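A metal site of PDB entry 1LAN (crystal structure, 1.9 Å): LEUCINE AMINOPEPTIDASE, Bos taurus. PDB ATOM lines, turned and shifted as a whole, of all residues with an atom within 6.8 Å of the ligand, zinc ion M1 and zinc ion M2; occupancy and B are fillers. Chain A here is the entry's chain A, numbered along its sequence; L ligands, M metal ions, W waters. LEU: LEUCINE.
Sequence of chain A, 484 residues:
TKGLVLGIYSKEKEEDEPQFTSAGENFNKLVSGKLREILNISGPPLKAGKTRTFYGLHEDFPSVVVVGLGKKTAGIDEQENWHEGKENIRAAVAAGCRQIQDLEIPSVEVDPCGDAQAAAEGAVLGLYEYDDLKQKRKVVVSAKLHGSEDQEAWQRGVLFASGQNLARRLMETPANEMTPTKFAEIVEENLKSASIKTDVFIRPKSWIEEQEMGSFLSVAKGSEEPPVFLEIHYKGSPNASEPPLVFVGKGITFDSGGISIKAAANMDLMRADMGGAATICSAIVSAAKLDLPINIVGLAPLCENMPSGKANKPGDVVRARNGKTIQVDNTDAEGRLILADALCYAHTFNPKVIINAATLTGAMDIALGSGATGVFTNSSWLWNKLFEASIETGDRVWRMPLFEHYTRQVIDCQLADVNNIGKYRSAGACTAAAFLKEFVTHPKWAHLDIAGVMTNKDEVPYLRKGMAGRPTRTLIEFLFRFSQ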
ATOM      1  N   LYS A 250     -16.472   9.084   4.544  1.00  0.00           N
ATOM      2  CA  LYS A 250     -15.321   8.206   4.265  1.00  0.00           C
ATOM      3  C   LYS A 250     -14.530   8.008   5.585  1.00  0.00           C
ATOM      4  O   LYS A 250     -14.029   8.987   6.165  1.00  0.00           O
ATOM      5  CB  LYS A 250     -14.407   8.845   3.207  1.00  0.00           C
ATOM      6  CG  LYS A 250     -13.066   8.154   3.022  1.00  0.00           C
ATOM      7  CD  LYS A 250     -12.117   9.004   2.170  1.00  0.00           C
ATOM      8  CE  LYS A 250     -10.742   8.334   2.044  1.00  0.00           C
ATOM      9  NZ  LYS A 250      -9.800   9.149   1.212  1.00  0.00           N
ATOM     10  N   ILE A 252     -11.456   6.166   6.421  1.00  0.00           N
ATOM     11  CA  ILE A 252     -10.194   5.451   6.316  1.00  0.00           C
ATOM     12  C   ILE A 252      -9.388   5.926   7.537  1.00  0.00           C
ATOM     13  O   ILE A 252      -8.953   7.069   7.586  1.00  0.00           O
ATOM     14  CB  ILE A 252      -9.466   5.786   4.993  1.00  0.00           C
ATOM     15  CG1 ILE A 252     -10.276   5.240   3.799  1.00  0.00           C
ATOM     16  CG2 ILE A 252      -8.015   5.214   4.992  1.00  0.00           C
ATOM     17  CD1 ILE A 252     -10.268   3.716   3.682  1.00  0.00           C
ATOM     18  N   ASP A 255      -4.413   5.851   5.831  1.00  0.00           N
ATOM     19  CA  ASP A 255      -4.166   5.620   4.404  1.00  0.00           C
ATOM     20  C   ASP A 255      -2.667   5.659   4.061  1.00  0.00           C
ATOM     21  O   ASP A 255      -2.045   6.731   4.012  1.00  0.00           O
ATOM     22  CB  ASP A 255      -4.925   6.662   3.567  1.00  0.00           C
ATOM     23  CG  ASP A 255      -4.897   6.338   2.065  1.00  0.00           C
ATOM     24  OD1 ASP A 255      -4.605   5.186   1.686  1.00  0.00           O
ATOM     25  OD2 ASP A 255      -5.188   7.259   1.274  1.00  0.00           O
ATOM     26  N   SER A 256      -2.097   4.473   3.829  1.00  0.00           N
ATOM     27  CA  SER A 256      -0.697   4.327   3.447  1.00  0.00           C
ATOM     28  C   SER A 256      -0.634   4.348   1.919  1.00  0.00           C
ATOM     29  O   SER A 256       0.441   4.512   1.317  1.00  0.00           O
ATOM     30  CB  SER A 256      -0.158   2.982   3.934  1.00  0.00           C
ATOM     31  OG  SER A 256      -0.671   1.898   3.168  1.00  0.00           O
ATOM     32  N   GLY A 257      -1.785   4.152   1.279  1.00  0.00           N
ATOM     33  CA  GLY A 257      -1.862   4.101  -0.172  1.00  0.00           C
ATOM     34  C   GLY A 257      -1.993   2.664  -0.678  1.00  0.00           C
ATOM     35  O   GLY A 257      -2.497   2.438  -1.800  1.00  0.00           O
ATOM     36  N   LYS A 262       2.195   5.476  -0.719  1.00  0.00           N
ATOM     37  CA  LYS A 262       2.474   6.902  -0.622  1.00  0.00           C
ATOM     38  C   LYS A 262       3.932   7.171  -0.259  1.00  0.00           C
ATOM     39  O   LYS A 262       4.620   6.299   0.266  1.00  0.00           O
ATOM     40  CB  LYS A 262       1.596   7.550   0.466  1.00  0.00           C
ATOM     41  CG  LYS A 262       0.098   7.612   0.176  1.00  0.00           C
ATOM     42  CD  LYS A 262      -0.636   8.232   1.376  1.00  0.00           C
ATOM     43  CE  LYS A 262      -2.139   8.346   1.118  1.00  0.00           C
ATOM     44  NZ  LYS A 262      -2.426   9.218  -0.055  1.00  0.00           N
ATOM     45  N   MET A 270      -2.160  11.307   7.316  1.00  0.00           N
ATOM     46  CA  MET A 270      -3.170  10.369   6.813  1.00  0.00           C
ATOM     47  C   MET A 270      -3.978   9.673   7.906  1.00  0.00           C
ATOM     48  O   MET A 270      -4.924   8.915   7.604  1.00  0.00           O
ATOM     49  CB  MET A 270      -2.576   9.351   5.812  1.00  0.00           C
ATOM     50  CG  MET A 270      -2.123   9.978   4.474  1.00  0.00           C
ATOM     51  SD  MET A 270      -3.404  10.911   3.598  1.00  0.00           S
ATOM     52  CE  MET A 270      -3.001  12.587   4.007  1.00  0.00           C
ATOM     53  N   ASP A 273      -7.551  10.668   7.512  1.00  0.00           N
ATOM     54  CA  ASP A 273      -8.270  10.295   6.295  1.00  0.00           C
ATOM     55  C   ASP A 273      -9.679   9.740   6.602  1.00  0.00           C
ATOM     56  O   ASP A 273     -10.357   9.160   5.737  1.00  0.00           O
ATOM     57  CB  ASP A 273      -7.431   9.309   5.475  1.00  0.00           C
ATOM     58  CG  ASP A 273      -7.756   9.344   3.980  1.00  0.00           C
ATOM     59  OD1 ASP A 273      -8.121  10.421   3.443  1.00  0.00           O
ATOM     60  OD2 ASP A 273      -7.637   8.277   3.339  1.00  0.00           O
ATOM     61  N   ASN A 305      -6.067   1.282   4.923  1.00  0.00           N
ATOM     62  CA  ASN A 305      -5.604   0.964   3.573  1.00  0.00           C
ATOM     63  C   ASN A 305      -4.101   0.681   3.733  1.00  0.00           C
ATOM     64  O   ASN A 305      -3.299   1.619   3.819  1.00  0.00           O
ATOM     65  CB  ASN A 305      -5.849   2.148   2.643  1.00  0.00           C
ATOM     66  CG  ASN A 305      -5.571   1.826   1.162  1.00  0.00           C
ATOM     67  OD1 ASN A 305      -5.250   2.728   0.369  1.00  0.00           O
ATOM     68  ND2 ASN A 305      -5.702   0.557   0.790  1.00  0.00           N
ATOM     69  N   ASN A 330      -5.451   2.286  -9.331  1.00  0.00           N
ATOM     70  CA  ASN A 330      -4.575   2.855  -8.307  1.00  0.00           C
ATOM     71  C   ASN A 330      -5.223   2.563  -6.935  1.00  0.00           C
ATOM     72  O   ASN A 330      -6.334   3.024  -6.660  1.00  0.00           O
ATOM     73  CB  ASN A 330      -4.398   4.372  -8.507  1.00  0.00           C
ATOM     74  CG  ASN A 330      -3.337   4.968  -7.573  1.00  0.00           C
ATOM     75  OD1 ASN A 330      -3.429   4.856  -6.361  1.00  0.00           O
ATOM     76  ND2 ASN A 330      -2.294   5.542  -8.157  1.00  0.00           N
ATOM     77  N   THR A 331      -4.540   1.784  -6.097  1.00  0.00           N
ATOM     78  CA  THR A 331      -5.069   1.419  -4.780  1.00  0.00           C
ATOM     79  C   THR A 331      -5.174   2.570  -3.768  1.00  0.00           C
ATOM     80  O   THR A 331      -5.807   2.421  -2.719  1.00  0.00           O
ATOM     81  CB  THR A 331      -4.279   0.226  -4.165  1.00  0.00           C
ATOM     82  OG1 THR A 331      -2.980   0.664  -3.752  1.00  0.00           O
ATOM     83  CG2 THR A 331      -4.084  -0.883  -5.202  1.00  0.00           C
ATOM     84  N   ASP A 332      -4.565   3.709  -4.080  1.00  0.00           N
ATOM     85  CA  ASP A 332      -4.591   4.883  -3.207  1.00  0.00           C
ATOM     86  C   ASP A 332      -5.838   5.740  -3.505  1.00  0.00           C
ATOM     87  O   ASP A 332      -6.074   6.758  -2.852  1.00  0.00           O
ATOM     88  CB  ASP A 332      -3.287   5.685  -3.344  1.00  0.00           C
ATOM     89  CG  ASP A 332      -3.071   6.712  -2.208  1.00  0.00           C
ATOM     90  OD1 ASP A 332      -3.771   6.694  -1.173  1.00  0.00           O
ATOM     91  OD2 ASP A 332      -2.167   7.551  -2.367  1.00  0.00           O
ATOM     92  N   ALA A 333      -6.618   5.355  -4.513  1.00  0.00           N
ATOM     93  CA  ALA A 333      -7.875   6.065  -4.802  1.00  0.00           C
ATOM     94  C   ALA A 333      -8.906   5.147  -4.136  1.00  0.00           C
ATOM     95  O   ALA A 333      -9.862   4.657  -4.771  1.00  0.00           O
ATOM     96  CB  ALA A 333      -8.113   6.137  -6.330  1.00  0.00           C
ATOM     97  N   GLU A 334      -8.698   4.894  -2.843  1.00  0.00           N
ATOM     98  CA  GLU A 334      -9.557   3.980  -2.076  1.00  0.00           C
ATOM     99  C   GLU A 334     -10.851   4.560  -1.509  1.00  0.00           C
ATOM    100  O   GLU A 334     -11.790   3.825  -1.242  1.00  0.00           O
ATOM    101  CB  GLU A 334      -8.735   3.265  -0.974  1.00  0.00           C
ATOM    102  CG  GLU A 334      -8.564   4.034   0.368  1.00  0.00           C
ATOM    103  CD  GLU A 334      -7.844   5.378   0.254  1.00  0.00           C
ATOM    104  OE1 GLU A 334      -6.881   5.505  -0.551  1.00  0.00           O
ATOM    105  OE2 GLU A 334      -8.213   6.333   1.002  1.00  0.00           O
ATOM    106  N   GLY A 335     -10.903   5.871  -1.315  1.00  0.00           N
ATOM    107  CA  GLY A 335     -12.094   6.473  -0.753  1.00  0.00           C
ATOM    108  C   GLY A 335     -13.302   6.324  -1.645  1.00  0.00           C
ATOM    109  O   GLY A 335     -14.402   6.031  -1.155  1.00  0.00           O
ATOM    110  N   ARG A 336     -13.109   6.481  -2.944  1.00  0.00           N
ATOM    111  CA  ARG A 336     -14.236   6.357  -3.872  1.00  0.00           C
ATOM    112  C   ARG A 336     -14.747   4.920  -3.909  1.00  0.00           C
ATOM    113  O   ARG A 336     -15.936   4.686  -4.146  1.00  0.00           O
ATOM    114  CB  ARG A 336     -13.913   6.910  -5.263  1.00  0.00           C
ATOM    115  CG  ARG A 336     -12.965   6.112  -6.130  1.00  0.00           C
ATOM    116  CD  ARG A 336     -12.506   6.982  -7.295  1.00  0.00           C
ATOM    117  NE  ARG A 336     -11.483   7.926  -6.869  1.00  0.00           N
ATOM    118  CZ  ARG A 336     -10.875   8.814  -7.655  1.00  0.00           C
ATOM    119  NH1 ARG A 336     -11.234   8.932  -8.916  1.00  0.00           N
ATOM    120  NH2 ARG A 336      -9.934   9.601  -7.158  1.00  0.00           N
ATOM    121  N   ALA A 358     -15.837  13.711   2.411  1.00  0.00           N
ATOM    122  CA  ALA A 358     -14.632  12.891   2.319  1.00  0.00           C
ATOM    123  C   ALA A 358     -13.360  13.697   2.084  1.00  0.00           C
ATOM    124  O   ALA A 358     -13.397  14.713   1.380  1.00  0.00           O
ATOM    125  CB  ALA A 358     -14.807  11.854   1.200  1.00  0.00           C
ATOM    126  N   THR A 359     -12.276  13.295   2.739  1.00  0.00           N
ATOM    127  CA  THR A 359     -10.948  13.908   2.554  1.00  0.00           C
ATOM    128  C   THR A 359     -10.492  13.082   1.341  1.00  0.00           C
ATOM    129  O   THR A 359      -9.646  12.198   1.443  1.00  0.00           O
ATOM    130  CB  THR A 359     -10.013  13.598   3.761  1.00  0.00           C
ATOM    131  OG1 THR A 359     -10.116  12.198   4.077  1.00  0.00           O
ATOM    132  CG2 THR A 359     -10.416  14.394   5.009  1.00  0.00           C
ATOM    133  N   LEU A 360     -11.097  13.374   0.188  1.00  0.00           N
ATOM    134  CA  LEU A 360     -10.892  12.566  -0.997  1.00  0.00           C
ATOM    135  C   LEU A 360      -9.704  12.736  -1.936  1.00  0.00           C
ATOM    136  O   LEU A 360      -9.048  11.757  -2.242  1.00  0.00           O
ATOM    137  CB  LEU A 360     -12.200  12.546  -1.811  1.00  0.00           C
ATOM    138  CG  LEU A 360     -12.482  11.390  -2.780  1.00  0.00           C
ATOM    139  CD1 LEU A 360     -12.593  10.072  -1.994  1.00  0.00           C
ATOM    140  CD2 LEU A 360     -13.779  11.647  -3.544  1.00  0.00           C
ATOM    141  N   THR A 361      -9.428  13.952  -2.391  1.00  0.00           N
ATOM    142  CA  THR A 361      -8.348  14.090  -3.364  1.00  0.00           C
ATOM    143  C   THR A 361      -7.324  15.143  -3.029  1.00  0.00           C
ATOM    144  O   THR A 361      -7.657  16.194  -2.481  1.00  0.00           O
ATOM    145  CB  THR A 361      -8.923  14.442  -4.755  1.00  0.00           C
ATOM    146  OG1 THR A 361      -9.558  15.724  -4.705  1.00  0.00           O
ATOM    147  CG2 THR A 361      -9.949  13.410  -5.216  1.00  0.00           C
ATOM    148  N   GLY A 362      -6.075  14.883  -3.425  1.00  0.00           N
ATOM    149  CA  GLY A 362      -5.023  15.865  -3.235  1.00  0.00           C
ATOM    150  C   GLY A 362      -5.336  17.026  -4.192  1.00  0.00           C
ATOM    151  O   GLY A 362      -5.002  18.187  -3.902  1.00  0.00           O
ATOM    152  N   ALA A 363      -6.021  16.716  -5.288  1.00  0.00           N
ATOM    153  CA  ALA A 363      -6.393  17.723  -6.287  1.00  0.00           C
ATOM    154  C   ALA A 363      -7.295  18.829  -5.709  1.00  0.00           C
ATOM    155  O   ALA A 363      -7.211  19.982  -6.135  1.00  0.00           O
ATOM    156  CB  ALA A 363      -7.079  17.069  -7.507  1.00  0.00           C
ATOM    157  N   ASP A 365      -7.134  19.994  -2.664  1.00  0.00           N
ATOM    158  CA  ASP A 365      -6.257  20.890  -1.915  1.00  0.00           C
ATOM    159  C   ASP A 365      -5.525  21.824  -2.888  1.00  0.00           C
ATOM    160  O   ASP A 365      -5.416  23.032  -2.664  1.00  0.00           O
ATOM    161  CB  ASP A 365      -5.270  20.106  -1.045  1.00  0.00           C
ATOM    162  CG  ASP A 365      -4.382  21.022  -0.217  1.00  0.00           C
ATOM    163  OD1 ASP A 365      -4.908  21.829   0.560  1.00  0.00           O
ATOM    164  OD2 ASP A 365      -3.146  20.989  -0.401  1.00  0.00           O
ATOM    165  N   ASP A 449     -15.825  17.502  -0.714  1.00  0.00           N
ATOM    166  CA  ASP A 449     -14.418  17.061  -0.689  1.00  0.00           C
ATOM    167  C   ASP A 449     -13.728  18.027   0.275  1.00  0.00           C
ATOM    168  O   ASP A 449     -13.513  19.190  -0.054  1.00  0.00           O
ATOM    169  CB  ASP A 449     -13.776  17.106  -2.081  1.00  0.00           C
ATOM    170  CG  ASP A 449     -12.438  16.365  -2.147  1.00  0.00           C
ATOM    171  OD1 ASP A 449     -11.793  16.171  -1.091  1.00  0.00           O
ATOM    172  OD2 ASP A 449     -12.027  15.966  -3.266  1.00  0.00           O
ATOM    173  N   ILE A 450     -13.375  17.515   1.451  1.00  0.00           N
ATOM    174  CA  ILE A 450     -12.746  18.320   2.517  1.00  0.00           C
ATOM    175  C   ILE A 450     -11.245  18.117   2.717  1.00  0.00           C
ATOM    176  O   ILE A 450     -10.688  18.509   3.738  1.00  0.00           O
ATOM    177  CB  ILE A 450     -13.482  18.056   3.863  1.00  0.00           C
ATOM    178  CG1 ILE A 450     -13.279  16.612   4.312  1.00  0.00           C
ATOM    179  CG2 ILE A 450     -14.992  18.327   3.700  1.00  0.00           C
ATOM    180  CD1 ILE A 450     -13.628  16.371   5.758  1.00  0.00           C
ATOM    181  N   ALA A 451     -10.572  17.549   1.704  1.00  0.00           N
ATOM    182  CA  ALA A 451      -9.136  17.292   1.754  1.00  0.00           C
ATOM    183  C   ALA A 451      -8.318  18.578   2.002  1.00  0.00           C
ATOM    184  O   ALA A 451      -7.345  18.563   2.756  1.00  0.00           O
ATOM    185  CB  ALA A 451      -8.657  16.596   0.479  1.00  0.00           C
ATOM    186  N   GLY A 452      -8.748  19.680   1.413  1.00  0.00           N
ATOM    187  CA  GLY A 452      -8.055  20.946   1.592  1.00  0.00           C
ATOM    188  C   GLY A 452      -8.277  21.634   2.937  1.00  0.00           C
ATOM    189  O   GLY A 452      -7.473  22.463   3.334  1.00  0.00           O
ATOM    190  N   MET A 454      -8.567  19.935   5.798  1.00  0.00           N
ATOM    191  CA  MET A 454      -8.269  18.895   6.788  1.00  0.00           C
ATOM    192  C   MET A 454      -7.475  19.454   7.968  1.00  0.00           C
ATOM    193  O   MET A 454      -7.725  19.127   9.128  1.00  0.00           O
ATOM    194  CB  MET A 454      -7.516  17.700   6.137  1.00  0.00           C
ATOM    195  CG  MET A 454      -7.470  16.443   6.998  1.00  0.00           C
ATOM    196  SD  MET A 454      -6.575  15.003   6.306  1.00  0.00           S
ATOM    197  CE  MET A 454      -4.917  15.545   6.527  1.00  0.00           C
HETATM  198  N   LEU L   1      -6.327  10.262   1.329  1.00  0.00           N
HETATM  199  CA  LEU L   1      -6.508  10.846  -0.016  1.00  0.00           C
HETATM  200  C   LEU L   1      -6.439   9.691  -1.063  1.00  0.00           C
HETATM  201  O   LEU L   1      -7.236   8.603  -0.665  1.00  0.00           O
HETATM  202  CB  LEU L   1      -5.394  11.848  -0.297  1.00  0.00           C
HETATM  203  CG  LEU L   1      -5.352  13.044   0.662  1.00  0.00           C
HETATM  204  CD1 LEU L   1      -4.477  14.173   0.209  1.00  0.00           C
HETATM  205  CD2 LEU L   1      -6.706  13.555   1.097  1.00  0.00           C
HETATM  206  OXT LEU L   1      -5.116   9.134  -1.023  1.00  0.00           O
HETATM  207 ZN    ZN M   1      -5.685   7.109  -0.750  1.00  0.00          ZN
HETATM  208 ZN    ZN M   2      -7.730   8.334   1.313  1.00  0.00          ZN
HETATM  209  O   HOH W   1      -4.552   9.798  -4.354  1.00  0.00           O
HETATM  210  O   HOH W   2      -9.446   8.382  -1.815  1.00  0.00           O
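OD1 of Asp 332 is bound to zinc ion M1.
The side-chain carboxylate (OE1) of Glu 334 binds zinc ion M1 (2.0 Å).
Zinc ion M1 is bound by OD2 of Asp 255, 2.1 Å away.
OXT of the ligand binds zinc ion M1 (2.1 Å).
Zinc ion M1 is bound by O of the ligand, 2.2 Å away.
The backbone carbonyl oxygen (O) of Asp 332 binds zinc ion M1, at 2.2 Å.
Zinc ion M1 has six donor atoms within binding distance.
Four residues have an atom within 4 Å of zinc ion M2: Lys 250, Asp 255, Asp 273 and Glu 334.
OXT of the ligand sits close to NZ of Lys 262 (2.9 Å).
The side-chain sulfur of Met 270 lies close to a nitrogen (N) of the ligand, 3.8 Å away.
Merely in contact with zinc ion M1: Lys 262.
Four residues have an atom within 4 Å of zinc ion M1: Asp 255, Lys 262, Asp 332 and Glu 334.
The nearest printed residue that does not touch zinc ion M1 is Ala 333 (4.3 Å).
Water W2 lies within hydrogen-bond range of N of Gly 335 (2.9 Å) and O of Leu 360 (3.4 Å).
The side-chain carboxylate (OD2) of Asp 332 lies within salt-bridge range of the side-chain amino group (NZ) of Lys 262, 2.9 Å away.
O of Gly 257 sits at hydrogen-bond distance from N of Asp 332, 3.3 Å away.
OD1 of Asn 330 lies within hydrogen-bond range of N of Asp 332, at 2.8 Å.
The side-chain carboxylate (OD2) of Asp 255 sits close to the side-chain amino group (NZ) of Lys 262 (3.6 Å).
The side-chain carboxylate of Asp 255 sits close to the side-chain amide oxygen of Asn 305, 2.9 Å away.
The side-chain amino group (NZ) of Lys 250 sits close to the backbone carbonyl oxygen (O) of Thr 359 (3.1 Å).
The backbone NH (N) of Lys 262 lies within hydrogen-bond range of the backbone carbonyl oxygen (O) of Ser 256 (2.9 Å).
The backbone NH of Leu 360 sits at hydrogen-bond distance from the side-chain carboxylate of Asp 449.
Thr 359 touches the ligand (O to CD2, 3.3 Å).
Leu 360 touches the ligand (O to CA, 3.5 Å).
CA of Gly 362 touches CD1 of the ligand, at 3.9 Å.
CB of Ala 451 touches CD2 of the ligand, 3.7 Å away.
11 residues have an atom within 4 Å of the ligand: Lys 250, Asp 255, Lys 262, Met 270, Asp 273, Asp 332, Glu 334, Thr 359, Leu 360, Gly 362 and Ala 451.
The nearest printed residue that does not touch the ligand is Thr 361 (4.4 Å).
The side-chain carboxylate (OD2) of Asp 273 binds zinc ion M2 (2.0 Å).
Zinc ion M2 is bound by O of the ligand (2.1 Å).
OE2 of Glu 334 binds zinc ion M2 (2.1 Å).
NZ of Lys 250 is bound to zinc ion M2 (2.2 Å).
N of the ligand binds zinc ion M2, at 2.4 Å.
Zinc ion M2 has five donor atoms within binding distance.
Slightly farther from zinc ion M2 lies OD2 of Asp 255 (2.8 Å).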
